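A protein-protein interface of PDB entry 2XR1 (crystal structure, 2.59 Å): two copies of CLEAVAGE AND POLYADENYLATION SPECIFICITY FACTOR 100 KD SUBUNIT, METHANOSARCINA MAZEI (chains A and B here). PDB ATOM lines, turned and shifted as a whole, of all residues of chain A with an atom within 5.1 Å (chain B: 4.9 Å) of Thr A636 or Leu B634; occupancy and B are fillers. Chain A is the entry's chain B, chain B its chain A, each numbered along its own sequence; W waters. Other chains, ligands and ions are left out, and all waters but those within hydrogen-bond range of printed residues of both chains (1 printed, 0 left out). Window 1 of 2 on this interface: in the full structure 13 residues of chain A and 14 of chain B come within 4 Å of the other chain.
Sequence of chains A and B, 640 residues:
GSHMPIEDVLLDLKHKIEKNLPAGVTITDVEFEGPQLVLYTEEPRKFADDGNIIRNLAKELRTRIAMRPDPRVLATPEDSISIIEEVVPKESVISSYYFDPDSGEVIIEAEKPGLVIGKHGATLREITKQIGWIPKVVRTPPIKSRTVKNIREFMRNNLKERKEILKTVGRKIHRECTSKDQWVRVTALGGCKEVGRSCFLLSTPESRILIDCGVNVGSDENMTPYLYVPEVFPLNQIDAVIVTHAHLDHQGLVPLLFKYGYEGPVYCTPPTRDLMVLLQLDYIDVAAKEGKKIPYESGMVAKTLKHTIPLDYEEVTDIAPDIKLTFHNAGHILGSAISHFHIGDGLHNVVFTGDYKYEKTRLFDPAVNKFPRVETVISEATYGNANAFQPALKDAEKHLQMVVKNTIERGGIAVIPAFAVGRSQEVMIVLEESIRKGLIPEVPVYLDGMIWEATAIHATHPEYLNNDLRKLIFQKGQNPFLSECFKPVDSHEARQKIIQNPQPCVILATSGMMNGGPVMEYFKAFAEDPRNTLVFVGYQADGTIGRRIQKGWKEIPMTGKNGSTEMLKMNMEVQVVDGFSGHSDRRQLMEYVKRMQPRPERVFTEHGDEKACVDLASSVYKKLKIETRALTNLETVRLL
The side-chain carboxylate of Glu B635 lies within hydrogen-bond range of the backbone NH of Arg A638, at 2.8 Å. The backbone carbonyl oxygen (O) of Asn B633 lies within hydrogen-bond range of the guanidinium group (NH1) of Arg A638 (3.0 Å). O of Thr A636 sits at hydrogen-bond distance from N of Thr B636, 3.0 Å away. NH1 of Arg A185 is in hydrogen-bond range of O of Leu B634, at 3.0 Å.
Leu A634 touches Thr B636, and with the chains exchanged Thr A636 touches Leu B634. Glu A635 touches Thr B636, and with the chains exchanged Thr A636 touches Glu B635. Thr B636 touches its own counterpart, Thr A636.
Hydrophobic or aromatic side chains of chain A that line the printed part of chain B: Trp A183 and Val A637. Printed residues of chain B that touch a printed residue of chain A: Tyr B226, Val B229, Asn B633, Leu B634, Glu B635 and Thr B636.
Water W1 lies within hydrogen-bond range of ND2 of Asn B633 (2.8 Å), OH of Tyr B226 (2.9 Å) and NH1 of Arg A638 (3.2 Å).
The backbone carbonyl oxygen (O) of Ala B188 sits at hydrogen-bond distance from the backbone NH (N) of Leu B634 (2.7 Å). O of Leu B189 is in hydrogen-bond range of N of Tyr B226 (2.9 Å). N of Val A637 is in hydrogen-bond range of O of Val A186, 2.9 Å away. N of Ala B188 sits at hydrogen-bond distance from O of Glu B635. The side-chain hydroxyl of Thr B636 is in hydrogen-bond range of the side-chain hydroxyl of Thr B187 (2.6 Å). The side-chain hydroxyl (OG1) of Thr A187 is in hydrogen-bond range of the side-chain hydroxyl (OG1) of Thr A636.
Among the printed residues, pairs that only touch across the chains: Thr A636 with Glu B635 (3.1 Å), Glu A635 with Thr B636 (3.2 Å), Val A637 with Glu B635 (3.5 Å), Arg A638 with Tyr B226 (3.6 Å), Trp A183 with Leu B634 (3.7 Å), Trp A183 with Tyr B226 (3.8 Å), Trp A183 with Val B229 (3.8 Å), Leu A634 with Thr B636 (3.9 Å), Thr A636 with Leu B634 (3.9 Å) and Arg A185 with Val B229 (3.9 Å).
Val A186 touches none of the printed residues of chain B. Printed residues of chain B within 4 Å of Leu A634: Thr B636 (3.9 Å). Of chain B, only Leu B634 (3.9 Å), Glu B635 (3.1 Å) and Thr B636 (3.0 Å) come within 4 Å of Thr A636. Of the printed residues of chain B, Val A637 touches Glu B635 (3.5 Å). Ala B188 touches none of the printed residues of chain A. Of the printed residues of chain A, Tyr B226 touches Trp A183 and Arg A638. Of the printed residues of chain A, Leu B634 touches Trp A183 (3.7 Å), Arg A185 (3.0 Å) and Thr A636 (3.9 Å). Of the printed residues of chain A, Glu B635 touches Thr A636 (3.1 Å), Val A637 (3.5 Å) and Arg A638 (2.8 Å). Of the printed residues of chain A, Thr B636 touches Leu A634 (3.9 Å), Glu A635 (3.2 Å) and Thr A636 (3.0 Å). The nearest printed residue of chain B that does not touch Thr A636 is Thr B187 (6.0 Å). The nearest printed residue of chain A that does not touch Tyr B226 is Arg A185 (7.4 Å).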
ATOM      1  N   TRP A 183      -0.207  18.445  26.654  1.00  0.00           N
ATOM      2  CA  TRP A 183      -1.158  18.435  27.734  1.00  0.00           C
ATOM      3  C   TRP A 183      -0.928  17.181  28.570  1.00  0.00           C
ATOM      4  O   TRP A 183      -0.232  16.242  28.145  1.00  0.00           O
ATOM      5  CB  TRP A 183      -2.600  18.510  27.250  1.00  0.00           C
ATOM      6  CG  TRP A 183      -2.965  17.661  26.103  1.00  0.00           C
ATOM      7  CD1 TRP A 183      -3.134  18.064  24.833  1.00  0.00           C
ATOM      8  CD2 TRP A 183      -3.288  16.268  26.127  1.00  0.00           C
ATOM      9  NE1 TRP A 183      -3.515  17.024  24.051  1.00  0.00           N
ATOM     10  CE2 TRP A 183      -3.600  15.899  24.831  1.00  0.00           C
ATOM     11  CE3 TRP A 183      -3.337  15.305  27.120  1.00  0.00           C
ATOM     12  CZ2 TRP A 183      -3.939  14.606  24.497  1.00  0.00           C
ATOM     13  CZ3 TRP A 183      -3.640  14.023  26.782  1.00  0.00           C
ATOM     14  CH2 TRP A 183      -3.967  13.690  25.483  1.00  0.00           C
ATOM     15  N   ARG A 185      -3.322  14.756  31.493  1.00  0.00           N
ATOM     16  CA  ARG A 185      -4.557  14.547  32.206  1.00  0.00           C
ATOM     17  C   ARG A 185      -4.628  13.215  32.904  1.00  0.00           C
ATOM     18  O   ARG A 185      -3.928  12.315  32.576  1.00  0.00           O
ATOM     19  CB  ARG A 185      -5.714  14.740  31.288  1.00  0.00           C
ATOM     20  CG  ARG A 185      -5.610  13.995  30.025  1.00  0.00           C
ATOM     21  CD  ARG A 185      -6.701  14.444  29.086  1.00  0.00           C
ATOM     22  NE  ARG A 185      -6.851  13.428  28.072  1.00  0.00           N
ATOM     23  CZ  ARG A 185      -7.978  13.063  27.497  1.00  0.00           C
ATOM     24  NH1 ARG A 185      -9.139  13.623  27.805  1.00  0.00           N
ATOM     25  NH2 ARG A 185      -7.922  12.112  26.596  1.00  0.00           N
ATOM     26  N   VAL A 186      -5.476  13.121  33.904  1.00  0.00           N
ATOM     27  CA  VAL A 186      -5.700  11.891  34.655  1.00  0.00           C
ATOM     28  C   VAL A 186      -7.168  11.490  34.584  1.00  0.00           C
ATOM     29  O   VAL A 186      -8.027  12.311  34.930  1.00  0.00           O
ATOM     30  CB  VAL A 186      -5.452  12.140  36.110  1.00  0.00           C
ATOM     31  CG1 VAL A 186      -5.782  10.891  36.893  1.00  0.00           C
ATOM     32  CG2 VAL A 186      -4.031  12.638  36.336  1.00  0.00           C
ATOM     33  N   THR A 187      -7.455  10.264  34.118  1.00  0.00           N
ATOM     34  CA  THR A 187      -8.807   9.699  34.121  1.00  0.00           C
ATOM     35  C   THR A 187      -8.852   8.669  35.223  1.00  0.00           C
ATOM     36  O   THR A 187      -7.891   7.944  35.405  1.00  0.00           O
ATOM     37  CB  THR A 187      -9.184   9.000  32.789  1.00  0.00           C
ATOM     38  OG1 THR A 187      -9.048   9.898  31.689  1.00  0.00           O
ATOM     39  CG2 THR A 187     -10.645   8.508  32.809  1.00  0.00           C
ATOM     40  N   GLU A 231     -11.049   5.057  26.801  1.00  0.00           N
ATOM     41  CA  GLU A 231      -9.755   5.533  27.292  1.00  0.00           C
ATOM     42  C   GLU A 231      -8.781   4.440  27.580  1.00  0.00           C
ATOM     43  O   GLU A 231      -7.620   4.722  27.755  1.00  0.00           O
ATOM     44  CB  GLU A 231      -9.922   6.291  28.626  1.00  0.00           C
ATOM     45  CG  GLU A 231     -10.772   7.527  28.567  1.00  0.00           C
ATOM     46  CD  GLU A 231     -12.265   7.256  28.648  1.00  0.00           C
ATOM     47  OE1 GLU A 231     -12.819   6.437  27.885  1.00  0.00           O
ATOM     48  OE2 GLU A 231     -12.914   7.888  29.461  1.00  0.00           O
ATOM     49  N   LEU A 634     -14.534   7.793  36.488  1.00  0.00           N
ATOM     50  CA  LEU A 634     -14.884   8.107  35.099  1.00  0.00           C
ATOM     51  C   LEU A 634     -14.812   9.556  34.705  1.00  0.00           C
ATOM     52  O   LEU A 634     -15.133   9.861  33.582  1.00  0.00           O
ATOM     53  CB  LEU A 634     -16.219   7.489  34.630  1.00  0.00           C
ATOM     54  CG  LEU A 634     -16.293   5.964  34.630  1.00  0.00           C
ATOM     55  CD1 LEU A 634     -17.674   5.540  34.273  1.00  0.00           C
ATOM     56  CD2 LEU A 634     -15.260   5.349  33.673  1.00  0.00           C
ATOM     57  N   GLU A 635     -14.361  10.425  35.596  1.00  0.00           N
ATOM     58  CA  GLU A 635     -14.014  11.806  35.272  1.00  0.00           C
ATOM     59  C   GLU A 635     -12.551  11.912  34.875  1.00  0.00           C
ATOM     60  O   GLU A 635     -11.739  11.085  35.259  1.00  0.00           O
ATOM     61  CB  GLU A 635     -14.299  12.719  36.468  1.00  0.00           C
ATOM     62  CG  GLU A 635     -15.788  12.713  36.874  1.00  0.00           C
ATOM     63  CD  GLU A 635     -16.338  14.042  37.490  1.00  0.00           C
ATOM     64  OE1 GLU A 635     -15.635  14.642  38.330  1.00  0.00           O
ATOM     65  OE2 GLU A 635     -17.489  14.468  37.145  1.00  0.00           O
ATOM     66  N   THR A 636     -12.219  12.883  34.042  1.00  0.00           N
ATOM     67  CA  THR A 636     -10.851  13.129  33.631  1.00  0.00           C
ATOM     68  C   THR A 636     -10.554  14.582  33.969  1.00  0.00           C
ATOM     69  O   THR A 636     -11.265  15.482  33.613  1.00  0.00           O
ATOM     70  CB  THR A 636     -10.598  12.912  32.099  1.00  0.00           C
ATOM     71  OG1 THR A 636     -10.976  11.598  31.738  1.00  0.00           O
ATOM     72  CG2 THR A 636      -9.096  13.057  31.729  1.00  0.00           C
ATOM     73  N   VAL A 637      -9.457  14.796  34.648  1.00  0.00           N
ATOM     74  CA  VAL A 637      -9.024  16.108  35.025  1.00  0.00           C
ATOM     75  C   VAL A 637      -7.762  16.513  34.234  1.00  0.00           C
ATOM     76  O   VAL A 637      -6.838  15.718  34.044  1.00  0.00           O
ATOM     77  CB  VAL A 637      -8.695  16.059  36.489  1.00  0.00           C
ATOM     78  CG1 VAL A 637      -7.767  17.164  36.829  1.00  0.00           C
ATOM     79  CG2 VAL A 637      -9.966  16.118  37.300  1.00  0.00           C
ATOM     80  N   ARG A 638      -7.718  17.756  33.785  1.00  0.00           N
ATOM     81  CA  ARG A 638      -6.551  18.247  33.057  1.00  0.00           C
ATOM     82  C   ARG A 638      -5.570  18.944  33.993  1.00  0.00           C
ATOM     83  O   ARG A 638      -5.942  19.768  34.813  1.00  0.00           O
ATOM     84  CB  ARG A 638      -6.962  19.175  31.956  1.00  0.00           C
ATOM     85  CG  ARG A 638      -5.833  19.551  31.037  1.00  0.00           C
ATOM     86  CD  ARG A 638      -6.382  20.295  29.866  1.00  0.00           C
ATOM     87  NE  ARG A 638      -5.339  20.828  29.030  1.00  0.00           N
ATOM     88  CZ  ARG A 638      -5.588  21.510  27.931  1.00  0.00           C
ATOM     89  NH1 ARG A 638      -6.844  21.753  27.533  1.00  0.00           N
ATOM     90  NH2 ARG A 638      -4.567  21.912  27.193  1.00  0.00           N
ATOM     91  N   THR B 187     -17.458  14.714  27.862  1.00  0.00           N
ATOM     92  CA  THR B 187     -16.060  15.127  27.659  1.00  0.00           C
ATOM     93  C   THR B 187     -16.046  16.349  26.751  1.00  0.00           C
ATOM     94  O   THR B 187     -16.765  16.392  25.764  1.00  0.00           O
ATOM     95  CB  THR B 187     -15.180  14.004  27.024  1.00  0.00           C
ATOM     96  OG1 THR B 187     -15.268  12.802  27.792  1.00  0.00           O
ATOM     97  CG2 THR B 187     -13.705  14.409  27.000  1.00  0.00           C
ATOM     98  N   ALA B 188     -15.224  17.333  27.075  1.00  0.00           N
ATOM     99  CA  ALA B 188     -15.096  18.529  26.252  1.00  0.00           C
ATOM    100  C   ALA B 188     -13.861  18.409  25.353  1.00  0.00           C
ATOM    101  O   ALA B 188     -12.786  18.089  25.821  1.00  0.00           O
ATOM    102  CB  ALA B 188     -14.966  19.751  27.135  1.00  0.00           C
ATOM    103  N   LEU B 189     -14.023  18.696  24.069  1.00  0.00           N
ATOM    104  CA  LEU B 189     -12.928  18.610  23.106  1.00  0.00           C
ATOM    105  C   LEU B 189     -12.584  19.948  22.463  1.00  0.00           C
ATOM    106  O   LEU B 189     -11.611  20.044  21.717  1.00  0.00           O
ATOM    107  CB  LEU B 189     -13.301  17.608  22.037  1.00  0.00           C
ATOM    108  CG  LEU B 189     -13.637  16.210  22.570  1.00  0.00           C
ATOM    109  CD1 LEU B 189     -14.353  15.401  21.535  1.00  0.00           C
ATOM    110  CD2 LEU B 189     -12.327  15.529  23.008  1.00  0.00           C
ATOM    111  N   TYR B 226      -9.679  18.907  19.930  1.00  0.00           N
ATOM    112  CA  TYR B 226      -8.835  17.754  20.170  1.00  0.00           C
ATOM    113  C   TYR B 226      -9.533  16.474  19.683  1.00  0.00           C
ATOM    114  O   TYR B 226     -10.011  15.697  20.472  1.00  0.00           O
ATOM    115  CB  TYR B 226      -8.455  17.638  21.657  1.00  0.00           C
ATOM    116  CG  TYR B 226      -7.674  18.811  22.200  1.00  0.00           C
ATOM    117  CD1 TYR B 226      -6.300  18.856  22.112  1.00  0.00           C
ATOM    118  CD2 TYR B 226      -8.314  19.876  22.780  1.00  0.00           C
ATOM    119  CE1 TYR B 226      -5.597  19.923  22.590  1.00  0.00           C
ATOM    120  CE2 TYR B 226      -7.615  20.955  23.261  1.00  0.00           C
ATOM    121  CZ  TYR B 226      -6.262  20.969  23.172  1.00  0.00           C
ATOM    122  OH  TYR B 226      -5.567  22.032  23.688  1.00  0.00           O
ATOM    123  N   VAL B 229      -7.851  12.086  20.309  1.00  0.00           N
ATOM    124  CA  VAL B 229      -7.717  11.443  21.616  1.00  0.00           C
ATOM    125  C   VAL B 229      -8.531  10.163  21.689  1.00  0.00           C
ATOM    126  O   VAL B 229      -9.527  10.032  21.001  1.00  0.00           O
ATOM    127  CB  VAL B 229      -8.226  12.383  22.735  1.00  0.00           C
ATOM    128  CG1 VAL B 229      -7.253  13.550  22.893  1.00  0.00           C
ATOM    129  CG2 VAL B 229      -9.669  12.842  22.447  1.00  0.00           C
ATOM    130  N   THR B 632     -13.481  22.627  31.157  1.00  0.00           N
ATOM    131  CA  THR B 632     -12.121  22.789  30.617  1.00  0.00           C
ATOM    132  C   THR B 632     -11.954  21.804  29.471  1.00  0.00           C
ATOM    133  O   THR B 632     -12.444  20.698  29.548  1.00  0.00           O
ATOM    134  CB  THR B 632     -11.045  22.537  31.712  1.00  0.00           C
ATOM    135  OG1 THR B 632     -11.070  23.611  32.654  1.00  0.00           O
ATOM    136  CG2 THR B 632      -9.619  22.425  31.135  1.00  0.00           C
ATOM    137  N   ASN B 633     -11.275  22.217  28.397  1.00  0.00           N
ATOM    138  CA  ASN B 633     -11.036  21.315  27.292  1.00  0.00           C
ATOM    139  C   ASN B 633     -10.262  20.129  27.816  1.00  0.00           C
ATOM    140  O   ASN B 633      -9.294  20.276  28.584  1.00  0.00           O
ATOM    141  CB  ASN B 633     -10.243  21.966  26.164  1.00  0.00           C
ATOM    142  CG  ASN B 633     -11.038  22.979  25.366  1.00  0.00           C
ATOM    143  OD1 ASN B 633     -12.267  23.004  25.371  1.00  0.00           O
ATOM    144  ND2 ASN B 633     -10.304  23.850  24.675  1.00  0.00           N
ATOM    145  N   LEU B 634     -10.737  18.953  27.412  1.00  0.00           N
ATOM    146  CA  LEU B 634     -10.161  17.625  27.709  1.00  0.00           C
ATOM    147  C   LEU B 634     -10.492  17.061  29.080  1.00  0.00           C
ATOM    148  O   LEU B 634     -10.015  15.994  29.390  1.00  0.00           O
ATOM    149  CB  LEU B 634      -8.637  17.575  27.457  1.00  0.00           C
ATOM    150  CG  LEU B 634      -8.181  17.822  26.002  1.00  0.00           C
ATOM    151  CD1 LEU B 634      -6.670  17.781  25.916  1.00  0.00           C
ATOM    152  CD2 LEU B 634      -8.786  16.827  25.003  1.00  0.00           C
ATOM    153  N   GLU B 635     -11.316  17.745  29.877  1.00  0.00           N
ATOM    154  CA  GLU B 635     -11.846  17.195  31.124  1.00  0.00           C
ATOM    155  C   GLU B 635     -13.115  16.417  30.807  1.00  0.00           C
ATOM    156  O   GLU B 635     -13.767  16.665  29.784  1.00  0.00           O
ATOM    157  CB  GLU B 635     -12.094  18.300  32.163  1.00  0.00           C
ATOM    158  CG  GLU B 635     -10.788  19.081  32.548  1.00  0.00           C
ATOM    159  CD  GLU B 635     -10.769  19.671  33.978  1.00  0.00           C
ATOM    160  OE1 GLU B 635     -11.769  20.323  34.370  1.00  0.00           O
ATOM    161  OE2 GLU B 635      -9.739  19.499  34.700  1.00  0.00           O
ATOM    162  N   THR B 636     -13.445  15.418  31.619  1.00  0.00           N
ATOM    163  CA  THR B 636     -14.701  14.707  31.454  1.00  0.00           C
ATOM    164  C   THR B 636     -15.354  14.804  32.771  1.00  0.00           C
ATOM    165  O   THR B 636     -14.709  14.573  33.766  1.00  0.00           O
ATOM    166  CB  THR B 636     -14.526  13.183  31.087  1.00  0.00           C
ATOM    167  OG1 THR B 636     -13.780  13.056  29.880  1.00  0.00           O
ATOM    168  CG2 THR B 636     -15.862  12.480  30.847  1.00  0.00           C
HETATM  169  O   HOH W   1      -7.511  23.741  25.085  1.00  0.00           O
